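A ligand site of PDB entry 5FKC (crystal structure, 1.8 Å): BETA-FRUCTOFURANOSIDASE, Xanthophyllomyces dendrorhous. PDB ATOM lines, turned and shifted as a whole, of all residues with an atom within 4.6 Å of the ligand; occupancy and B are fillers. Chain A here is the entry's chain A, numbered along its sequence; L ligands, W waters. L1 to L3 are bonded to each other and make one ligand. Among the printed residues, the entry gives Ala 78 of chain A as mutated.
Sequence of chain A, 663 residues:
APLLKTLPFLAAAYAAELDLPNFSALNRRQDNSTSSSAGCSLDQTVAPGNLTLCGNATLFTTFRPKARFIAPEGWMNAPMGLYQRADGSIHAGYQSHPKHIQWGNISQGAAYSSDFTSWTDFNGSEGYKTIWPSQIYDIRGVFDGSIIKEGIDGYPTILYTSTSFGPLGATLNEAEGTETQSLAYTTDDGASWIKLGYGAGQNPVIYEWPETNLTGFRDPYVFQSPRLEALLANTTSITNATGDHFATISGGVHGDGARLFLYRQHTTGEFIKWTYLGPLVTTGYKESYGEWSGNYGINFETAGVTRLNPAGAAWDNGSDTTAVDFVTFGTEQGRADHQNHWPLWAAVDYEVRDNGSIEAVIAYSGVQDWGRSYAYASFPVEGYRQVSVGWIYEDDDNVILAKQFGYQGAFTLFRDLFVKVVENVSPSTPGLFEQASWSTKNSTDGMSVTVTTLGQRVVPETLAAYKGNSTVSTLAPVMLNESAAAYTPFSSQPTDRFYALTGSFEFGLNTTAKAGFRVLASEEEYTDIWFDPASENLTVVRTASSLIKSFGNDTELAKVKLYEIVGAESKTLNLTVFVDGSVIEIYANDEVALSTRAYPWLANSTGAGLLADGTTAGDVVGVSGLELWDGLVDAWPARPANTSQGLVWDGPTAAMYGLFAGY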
ATOM      1  N   ASN A  77     -15.002 -36.061  26.327  1.00  0.00           N
ATOM      2  CA  ASN A  77     -14.951 -34.816  25.587  1.00  0.00           C
ATOM      3  C   ASN A  77     -14.004 -34.911  24.381  1.00  0.00           C
ATOM      4  O   ASN A  77     -14.262 -35.709  23.481  1.00  0.00           O
ATOM      5  CB  ASN A  77     -14.821 -33.548  26.484  1.00  0.00           C
ATOM      6  CG  ASN A  77     -13.602 -33.535  27.402  1.00  0.00           C
ATOM      7  OD1 ASN A  77     -13.467 -34.349  28.304  1.00  0.00           O
ATOM      8  ND2 ASN A  77     -12.746 -32.537  27.204  1.00  0.00           N
ATOM      9  N   ALA A  78     -12.929 -34.123  24.345  1.00  0.00           N
ATOM     10  CA  ALA A  78     -12.137 -33.909  23.130  1.00  0.00           C
ATOM     11  C   ALA A  78     -11.526 -35.187  22.572  1.00  0.00           C
ATOM     12  O   ALA A  78     -10.977 -35.986  23.325  1.00  0.00           O
ATOM     13  CB  ALA A  78     -11.015 -32.922  23.417  1.00  0.00           C
ATOM     14  N   GLN A  95     -10.685 -37.764  25.542  1.00  0.00           N
ATOM     15  CA  GLN A  95     -10.739 -37.362  26.932  1.00  0.00           C
ATOM     16  C   GLN A  95     -11.893 -38.137  27.581  1.00  0.00           C
ATOM     17  O   GLN A  95     -13.011 -38.083  27.063  1.00  0.00           O
ATOM     18  CB  GLN A  95     -10.967 -35.849  27.039  1.00  0.00           C
ATOM     19  CG  GLN A  95      -9.783 -35.021  26.537  1.00  0.00           C
ATOM     20  CD  GLN A  95      -8.667 -34.939  27.553  1.00  0.00           C
ATOM     21  OE1 GLN A  95      -8.692 -34.102  28.432  1.00  0.00           O
ATOM     22  NE2 GLN A  95      -7.675 -35.834  27.428  1.00  0.00           N
ATOM     23  N   TRP A 103     -16.682 -34.086  34.048  1.00  0.00           N
ATOM     24  CA  TRP A 103     -15.244 -34.178  33.814  1.00  0.00           C
ATOM     25  C   TRP A 103     -14.458 -34.413  35.100  1.00  0.00           C
ATOM     26  O   TRP A 103     -14.815 -33.920  36.166  1.00  0.00           O
ATOM     27  CB  TRP A 103     -14.815 -32.861  33.158  1.00  0.00           C
ATOM     28  CG  TRP A 103     -13.395 -32.688  32.720  1.00  0.00           C
ATOM     29  CD1 TRP A 103     -12.919 -32.811  31.448  1.00  0.00           C
ATOM     30  CD2 TRP A 103     -12.287 -32.272  33.520  1.00  0.00           C
ATOM     31  NE1 TRP A 103     -11.581 -32.512  31.405  1.00  0.00           N
ATOM     32  CE2 TRP A 103     -11.159 -32.177  32.664  1.00  0.00           C
ATOM     33  CE3 TRP A 103     -12.133 -31.955  34.873  1.00  0.00           C
ATOM     34  CZ2 TRP A 103      -9.907 -31.798  33.120  1.00  0.00           C
ATOM     35  CZ3 TRP A 103     -10.881 -31.575  35.329  1.00  0.00           C
ATOM     36  CH2 TRP A 103      -9.782 -31.488  34.450  1.00  0.00           C
ATOM     37  N   ILE A 106      -8.973 -36.822  34.148  1.00  0.00           N
ATOM     38  CA  ILE A 106      -9.225 -36.985  32.733  1.00  0.00           C
ATOM     39  C   ILE A 106      -8.105 -37.828  32.113  1.00  0.00           C
ATOM     40  O   ILE A 106      -6.932 -37.656  32.417  1.00  0.00           O
ATOM     41  CB  ILE A 106      -9.505 -35.643  32.032  1.00  0.00           C
ATOM     42  CG1 ILE A 106     -10.366 -35.864  30.775  1.00  0.00           C
ATOM     43  CG2 ILE A 106      -8.217 -34.884  31.724  1.00  0.00           C
ATOM     44  CD1 ILE A 106     -11.817 -36.224  31.056  1.00  0.00           C
ATOM     45  N   ARG A 140      -3.398 -34.210  37.833  1.00  0.00           N
ATOM     46  CA  ARG A 140      -4.611 -33.416  37.739  1.00  0.00           C
ATOM     47  C   ARG A 140      -5.378 -33.673  36.442  1.00  0.00           C
ATOM     48  O   ARG A 140      -6.494 -33.196  36.291  1.00  0.00           O
ATOM     49  CB  ARG A 140      -4.266 -31.933  37.908  1.00  0.00           C
ATOM     50  CG  ARG A 140      -5.458 -31.007  38.108  1.00  0.00           C
ATOM     51  CD  ARG A 140      -5.794 -30.177  36.895  1.00  0.00           C
ATOM     52  NE  ARG A 140      -6.743 -29.142  37.262  1.00  0.00           N
ATOM     53  CZ  ARG A 140      -6.438 -28.004  37.889  1.00  0.00           C
ATOM     54  NH1 ARG A 140      -5.173 -27.729  38.245  1.00  0.00           N
ATOM     55  NH2 ARG A 140      -7.401 -27.139  38.184  1.00  0.00           N
ATOM     56  N   PHE A 143      -4.503 -34.282  29.672  1.00  0.00           N
ATOM     57  CA  PHE A 143      -5.264 -33.437  28.745  1.00  0.00           C
ATOM     58  C   PHE A 143      -4.953 -33.855  27.292  1.00  0.00           C
ATOM     59  O   PHE A 143      -4.289 -34.879  27.057  1.00  0.00           O
ATOM     60  CB  PHE A 143      -4.940 -31.947  28.981  1.00  0.00           C
ATOM     61  CG  PHE A 143      -5.671 -31.302  30.129  1.00  0.00           C
ATOM     62  CD1 PHE A 143      -5.990 -31.991  31.291  1.00  0.00           C
ATOM     63  CD2 PHE A 143      -5.978 -29.947  30.063  1.00  0.00           C
ATOM     64  CE1 PHE A 143      -6.609 -31.355  32.353  1.00  0.00           C
ATOM     65  CE2 PHE A 143      -6.611 -29.301  31.123  1.00  0.00           C
ATOM     66  CZ  PHE A 143      -6.939 -30.019  32.270  1.00  0.00           C
ATOM     67  N   ASP A 144      -5.470 -33.101  26.333  1.00  0.00           N
ATOM     68  CA  ASP A 144      -5.300 -33.377  24.901  1.00  0.00           C
ATOM     69  C   ASP A 144      -3.810 -33.532  24.527  1.00  0.00           C
ATOM     70  O   ASP A 144      -2.922 -32.939  25.135  1.00  0.00           O
ATOM     71  CB  ASP A 144      -5.959 -32.231  24.107  1.00  0.00           C
ATOM     72  CG  ASP A 144      -6.045 -32.480  22.605  1.00  0.00           C
ATOM     73  OD1 ASP A 144      -5.972 -33.628  22.120  1.00  0.00           O
ATOM     74  OD2 ASP A 144      -6.256 -31.443  21.896  1.00  0.00           O
ATOM     75  N   LEU A 168      -6.470 -23.319  37.042  1.00  0.00           N
ATOM     76  CA  LEU A 168      -6.260 -23.653  35.645  1.00  0.00           C
ATOM     77  C   LEU A 168      -7.447 -23.101  34.869  1.00  0.00           C
ATOM     78  O   LEU A 168      -8.599 -23.505  35.094  1.00  0.00           O
ATOM     79  CB  LEU A 168      -6.144 -25.172  35.474  1.00  0.00           C
ATOM     80  CG  LEU A 168      -5.606 -25.707  34.125  1.00  0.00           C
ATOM     81  CD1 LEU A 168      -5.251 -27.184  34.262  1.00  0.00           C
ATOM     82  CD2 LEU A 168      -6.586 -25.486  32.990  1.00  0.00           C
ATOM     83  N   GLY A 169      -7.187 -22.155  33.969  1.00  0.00           N
ATOM     84  CA  GLY A 169      -8.250 -21.583  33.153  1.00  0.00           C
ATOM     85  C   GLY A 169      -7.946 -20.206  32.647  1.00  0.00           C
ATOM     86  O   GLY A 169      -7.190 -19.451  33.288  1.00  0.00           O
ATOM     87  N   LEU A 172      -8.924 -17.524  35.128  1.00  0.00           N
ATOM     88  CA  LEU A 172      -8.294 -17.641  36.436  1.00  0.00           C
ATOM     89  C   LEU A 172      -6.857 -17.155  36.352  1.00  0.00           C
ATOM     90  O   LEU A 172      -6.382 -16.782  35.286  1.00  0.00           O
ATOM     91  CB  LEU A 172      -8.337 -19.094  36.906  1.00  0.00           C
ATOM     92  CG  LEU A 172      -9.734 -19.688  37.046  1.00  0.00           C
ATOM     93  CD1 LEU A 172      -9.650 -21.149  37.467  1.00  0.00           C
ATOM     94  CD2 LEU A 172     -10.563 -18.885  38.054  1.00  0.00           C
ATOM     95  N   ARG A 218      -1.635 -25.402  26.485  1.00  0.00           N
ATOM     96  CA  ARG A 218      -2.046 -26.792  26.325  1.00  0.00           C
ATOM     97  C   ARG A 218      -2.334 -27.210  24.895  1.00  0.00           C
ATOM     98  O   ARG A 218      -2.287 -26.381  23.960  1.00  0.00           O
ATOM     99  CB  ARG A 218      -3.257 -27.083  27.226  1.00  0.00           C
ATOM    100  CG  ARG A 218      -4.492 -26.222  26.978  1.00  0.00           C
ATOM    101  CD  ARG A 218      -5.713 -26.799  27.708  1.00  0.00           C
ATOM    102  NE  ARG A 218      -6.825 -25.848  27.733  1.00  0.00           N
ATOM    103  CZ  ARG A 218      -6.898 -24.764  28.517  1.00  0.00           C
ATOM    104  NH1 ARG A 218      -5.935 -24.479  29.394  1.00  0.00           N
ATOM    105  NH2 ARG A 218      -7.938 -23.939  28.408  1.00  0.00           N
ATOM    106  N   ASP A 219      -2.613 -28.499  24.747  1.00  0.00           N
ATOM    107  CA  ASP A 219      -3.111 -29.087  23.514  1.00  0.00           C
ATOM    108  C   ASP A 219      -2.026 -29.074  22.430  1.00  0.00           C
ATOM    109  O   ASP A 219      -2.234 -28.531  21.345  1.00  0.00           O
ATOM    110  CB  ASP A 219      -4.409 -28.411  23.056  1.00  0.00           C
ATOM    111  CG  ASP A 219      -5.501 -28.404  24.137  1.00  0.00           C
ATOM    112  OD1 ASP A 219      -5.381 -29.179  25.112  1.00  0.00           O
ATOM    113  OD2 ASP A 219      -6.452 -27.611  24.003  1.00  0.00           O
ATOM    114  N   GLU A 301      -7.739 -23.097  22.090  1.00  0.00           N
ATOM    115  CA  GLU A 301      -7.627 -24.492  22.516  1.00  0.00           C
ATOM    116  C   GLU A 301      -7.604 -25.398  21.293  1.00  0.00           C
ATOM    117  O   GLU A 301      -8.083 -25.017  20.221  1.00  0.00           O
ATOM    118  CB  GLU A 301      -8.808 -24.879  23.400  1.00  0.00           C
ATOM    119  CG  GLU A 301      -8.954 -24.036  24.662  1.00  0.00           C
ATOM    120  CD  GLU A 301     -10.162 -24.434  25.466  1.00  0.00           C
ATOM    121  OE1 GLU A 301     -11.285 -24.394  24.924  1.00  0.00           O
ATOM    122  OE2 GLU A 301      -9.998 -24.760  26.649  1.00  0.00           O
ATOM    123  N   THR A 302      -7.091 -26.604  21.485  1.00  0.00           N
ATOM    124  CA  THR A 302      -7.067 -27.680  20.489  1.00  0.00           C
ATOM    125  C   THR A 302      -6.727 -27.215  19.079  1.00  0.00           C
ATOM    126  O   THR A 302      -7.332 -27.675  18.120  1.00  0.00           O
ATOM    127  CB  THR A 302      -8.389 -28.520  20.476  1.00  0.00           C
ATOM    128  OG1 THR A 302      -9.448 -27.785  19.846  1.00  0.00           O
ATOM    129  CG2 THR A 302      -8.807 -28.911  21.882  1.00  0.00           C
ATOM    130  N   GLU A 332     -12.244 -19.441  23.348  1.00  0.00           N
ATOM    131  CA  GLU A 332     -13.014 -19.358  24.573  1.00  0.00           C
ATOM    132  C   GLU A 332     -13.411 -17.922  24.906  1.00  0.00           C
ATOM    133  O   GLU A 332     -12.648 -16.991  24.676  1.00  0.00           O
ATOM    134  CB  GLU A 332     -12.205 -19.854  25.759  1.00  0.00           C
ATOM    135  CG  GLU A 332     -11.540 -21.197  25.588  1.00  0.00           C
ATOM    136  CD  GLU A 332     -11.166 -21.770  26.940  1.00  0.00           C
ATOM    137  OE1 GLU A 332     -12.038 -22.442  27.533  1.00  0.00           O
ATOM    138  OE2 GLU A 332     -10.018 -21.533  27.395  1.00  0.00           O
ATOM    139  N   HIS A 341     -17.797 -21.324  23.456  1.00  0.00           N
ATOM    140  CA  HIS A 341     -16.806 -21.990  22.624  1.00  0.00           C
ATOM    141  C   HIS A 341     -17.113 -21.902  21.129  1.00  0.00           C
ATOM    142  O   HIS A 341     -18.190 -22.326  20.695  1.00  0.00           O
ATOM    143  CB  HIS A 341     -16.720 -23.470  23.006  1.00  0.00           C
ATOM    144  CG  HIS A 341     -15.800 -23.763  24.138  1.00  0.00           C
ATOM    145  ND1 HIS A 341     -15.958 -24.860  24.965  1.00  0.00           N
ATOM    146  CD2 HIS A 341     -14.708 -23.112  24.600  1.00  0.00           C
ATOM    147  CE1 HIS A 341     -15.001 -24.882  25.868  1.00  0.00           C
ATOM    148  NE2 HIS A 341     -14.223 -23.833  25.673  1.00  0.00           N
ATOM    149  N   TYR A 374     -17.090 -28.925  19.353  1.00  0.00           N
ATOM    150  CA  TYR A 374     -15.873 -28.240  19.734  1.00  0.00           C
ATOM    151  C   TYR A 374     -14.738 -29.248  19.730  1.00  0.00           C
ATOM    152  O   TYR A 374     -14.984 -30.456  19.610  1.00  0.00           O
ATOM    153  CB  TYR A 374     -16.020 -27.643  21.136  1.00  0.00           C
ATOM    154  CG  TYR A 374     -14.984 -26.615  21.518  1.00  0.00           C
ATOM    155  CD1 TYR A 374     -14.844 -25.434  20.788  1.00  0.00           C
ATOM    156  CD2 TYR A 374     -14.136 -26.828  22.602  1.00  0.00           C
ATOM    157  CE1 TYR A 374     -13.900 -24.482  21.136  1.00  0.00           C
ATOM    158  CE2 TYR A 374     -13.187 -25.888  22.955  1.00  0.00           C
ATOM    159  CZ  TYR A 374     -13.072 -24.717  22.212  1.00  0.00           C
ATOM    160  OH  TYR A 374     -12.146 -23.770  22.566  1.00  0.00           O
ATOM    161  N   TRP A 391     -15.952 -33.128  18.957  1.00  0.00           N
ATOM    162  CA  TRP A 391     -16.779 -33.635  20.045  1.00  0.00           C
ATOM    163  C   TRP A 391     -18.092 -32.882  20.064  1.00  0.00           C
ATOM    164  O   TRP A 391     -18.086 -31.652  20.005  1.00  0.00           O
ATOM    165  CB  TRP A 391     -16.032 -33.449  21.355  1.00  0.00           C
ATOM    166  CG  TRP A 391     -16.829 -33.288  22.624  1.00  0.00           C
ATOM    167  CD1 TRP A 391     -17.607 -34.214  23.222  1.00  0.00           C
ATOM    168  CD2 TRP A 391     -16.817 -32.140  23.476  1.00  0.00           C
ATOM    169  NE1 TRP A 391     -18.111 -33.715  24.400  1.00  0.00           N
ATOM    170  CE2 TRP A 391     -17.639 -32.439  24.581  1.00  0.00           C
ATOM    171  CE3 TRP A 391     -16.199 -30.882  23.418  1.00  0.00           C
ATOM    172  CZ2 TRP A 391     -17.867 -31.534  25.615  1.00  0.00           C
ATOM    173  CZ3 TRP A 391     -16.427 -29.977  24.451  1.00  0.00           C
ATOM    174  CH2 TRP A 391     -17.253 -30.300  25.530  1.00  0.00           C
HETATM  175  C1  LIG L   1     -11.140 -28.200  25.337  1.00  0.00           C
HETATM  176  C2  LIG L   1     -10.274 -28.701  26.496  1.00  0.00           C
HETATM  177  C3  LIG L   1      -8.827 -28.824  26.003  1.00  0.00           C
HETATM  178  C4  LIG L   1      -8.216 -29.727  27.074  1.00  0.00           C
HETATM  179  C5  LIG L   1      -9.376 -30.697  27.337  1.00  0.00           C
HETATM  180  C6  LIG L   1      -9.470 -31.141  28.798  1.00  0.00           C
HETATM  181  O1  LIG L   1     -12.522 -28.048  25.673  1.00  0.00           O
HETATM  182  O2  LIG L   1     -10.335 -27.824  27.628  1.00  0.00           O
HETATM  183  O3  LIG L   1      -8.193 -27.555  25.851  1.00  0.00           O
HETATM  184  O4  LIG L   1      -7.031 -30.429  26.640  1.00  0.00           O
HETATM  185  O5  LIG L   1     -10.568 -30.028  26.920  1.00  0.00           O
HETATM  186  O6  LIG L   1     -10.340 -32.284  28.943  1.00  0.00           O
HETATM  187  C1  LG2 L   2     -11.526 -27.804  28.429  1.00  0.00           C
HETATM  188  C2  LG2 L   2     -12.095 -26.383  28.532  1.00  0.00           C
HETATM  189  C3  LG2 L   2     -11.183 -25.470  29.346  1.00  0.00           C
HETATM  190  C4  LG2 L   2     -10.968 -26.092  30.711  1.00  0.00           C
HETATM  191  C5  LG2 L   2     -10.430 -27.528  30.574  1.00  0.00           C
HETATM  192  C6  LG2 L   2     -10.408 -28.219  31.931  1.00  0.00           C
HETATM  193  O1  LG2 L   2     -12.334 -25.837  27.225  1.00  0.00           O
HETATM  194  O2  LG2 L   2     -11.783 -24.172  29.454  1.00  0.00           O
HETATM  195  O3  LG2 L   2     -10.042 -25.332  31.480  1.00  0.00           O
HETATM  196  O4  LG2 L   2     -11.249 -28.317  29.716  1.00  0.00           O
HETATM  197  O5  LG2 L   2     -11.715 -28.074  32.490  1.00  0.00           O
HETATM  198  C1  LG3 L   3     -11.919 -28.665  33.760  1.00  0.00           C
HETATM  199  C2  LG3 L   3     -13.397 -28.617  34.147  1.00  0.00           C
HETATM  200  C3  LG3 L   3     -13.847 -27.171  34.292  1.00  0.00           C
HETATM  201  C4  LG3 L   3     -12.953 -26.441  35.304  1.00  0.00           C
HETATM  202  C5  LG3 L   3     -11.465 -26.620  34.936  1.00  0.00           C
HETATM  203  C6  LG3 L   3     -10.478 -26.085  35.968  1.00  0.00           C
HETATM  204  O1  LG3 L   3     -14.170 -29.282  33.153  1.00  0.00           O
HETATM  205  O2  LG3 L   3     -15.236 -27.155  34.686  1.00  0.00           O
HETATM  206  O3  LG3 L   3     -13.241 -26.943  36.623  1.00  0.00           O
HETATM  207  O4  LG3 L   3     -11.144 -28.019  34.748  1.00  0.00           O
HETATM  208  O5  LG3 L   3     -10.647 -24.677  36.067  1.00  0.00           O
HETATM  209  O   HOH W   1     -14.129 -24.242  30.753  1.00  0.00           O
HETATM  210  O   HOH W   2     -13.502 -29.456  37.674  1.00  0.00           O
HETATM  211  O   HOH W   3     -12.503 -26.166  39.024  1.00  0.00           O
HETATM  212  O   HOH W   4      -8.837 -24.294  38.537  1.00  0.00           O
HETATM  213  O   HOH W   5      -9.672 -29.045  37.121  1.00  0.00           O
HETATM  214  O   HOH W   6      -9.755 -22.075  30.044  1.00  0.00           O
HETATM  215  O   HOH W   7     -16.836 -29.288  32.992  1.00  0.00           O
HETATM  216  O   HOH W   8     -11.108 -23.435  32.966  1.00  0.00           O
HETATM  217  O   HOH W   9     -12.911 -23.247  37.263  1.00  0.00           O
HETATM  218  O   HOH W  10     -13.554 -30.446  25.423  1.00  0.00           O
HETATM  219  O   HOH W  11     -13.913 -29.126  30.463  1.00  0.00           O
HETATM  220  O   HOH W  12     -15.777 -26.509  37.755  1.00  0.00           O
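OE1 of Gln 95 is in hydrogen-bond range of O6 of LIG L1, at 2.5 Å. An oxygen (O3) of LIG L1 is in hydrogen-bond range of the side-chain carboxylate (OD2) of Asp 219. O5 of LG3 L3 sits at hydrogen-bond distance from O of Leu 168 (2.6 Å). O2 of LG2 L2 lies within hydrogen-bond range of OE1 of Glu 332 (2.6 Å). The side-chain carboxylate (OE2) of Glu 301 sits at hydrogen-bond distance from an oxygen (O1) of LG2 L2, at 2.6 Å. The indole nitrogen of Trp 103 is in hydrogen-bond range of an oxygen (O6) of LIG L1 (2.8 Å). NE of Arg 218 sits at hydrogen-bond distance from O3 of LIG L1 (2.9 Å). ND2 of Asn 77 lies within hydrogen-bond range of O6 of LIG L1. An oxygen (O4) of LIG L1 is in hydrogen-bond range of the backbone NH of Asp 144 (3.1 Å). A ring nitrogen (NE2) of His 341 sits close to an oxygen (O1) of LG2 L2 (3.2 Å).
O of Gln 95 lies within hydrogen-bond range of N of Asn 77 (2.9 Å). N of Gln 95 lies within hydrogen-bond range of O of Ala 78 (2.9 Å). The side-chain carboxylate (OD2) of Asp 219 is in hydrogen-bond range of the backbone NH (N) of Thr 302. The side-chain carboxylate of Glu 332 is in salt-bridge range of the guanidinium group of Arg 218. The side-chain carboxylate (OE2) of Glu 301 lies within salt-bridge range of the guanidinium group (NH2) of Arg 218 (2.8 Å). The side-chain carboxylate (OE1) of Glu 301 sits at hydrogen-bond distance from a ring nitrogen (NE2) of His 341 (3.1 Å). OH of Tyr 374 is in hydrogen-bond range of OE1 of Glu 301, 2.6 Å away. The backbone carbonyl oxygen (O) of Tyr 374 is in hydrogen-bond range of the backbone NH (N) of Trp 391 (2.9 Å).
NH2 of Arg 140 touches C6 of LG3 L3 (3.9 Å). CB of Phe 143 touches O4 of LIG L1, 3.5 Å away. CD1 of Leu 172 touches O5 of LG3 L3, 3.9 Å away. CE2 of Tyr 374 touches O1 of LIG L1, at 3.5 Å. Hydrophobic or aromatic side chains within 4 Å of the ligand: Trp 103, Phe 143, Leu 168, Leu 172, His 341 and Tyr 374. Of the 19 residues printed, 14 come within 4 Å of the ligand. The nearest printed residue that does not touch the ligand is Ile 106 (4.02 Å).
Water W10 bridges an oxygen (O1) of LIG L1 (2.6 Å) and the side-chain amide nitrogen (ND2) of Asn 77 (2.9 Å). Water W8 lies within hydrogen-bond range of O3 of LG2 L2 and O of Leu 168. Water W5 lies within hydrogen-bond range of the guanidinium group of Arg 140 and an oxygen (O4) of LG3 L3. Water W6 lies within hydrogen-bond range of OE2 of Glu 332 (2.7 Å), O2 of LG2 L2 (3.0 Å) and NH2 of Arg 218 (3.1 Å). Water W4 lies within hydrogen-bond range of N of Leu 168 (3.0 Å), O5 of LG3 L3 (3.1 Å) and NH2 of Arg 140 (3.2 Å).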
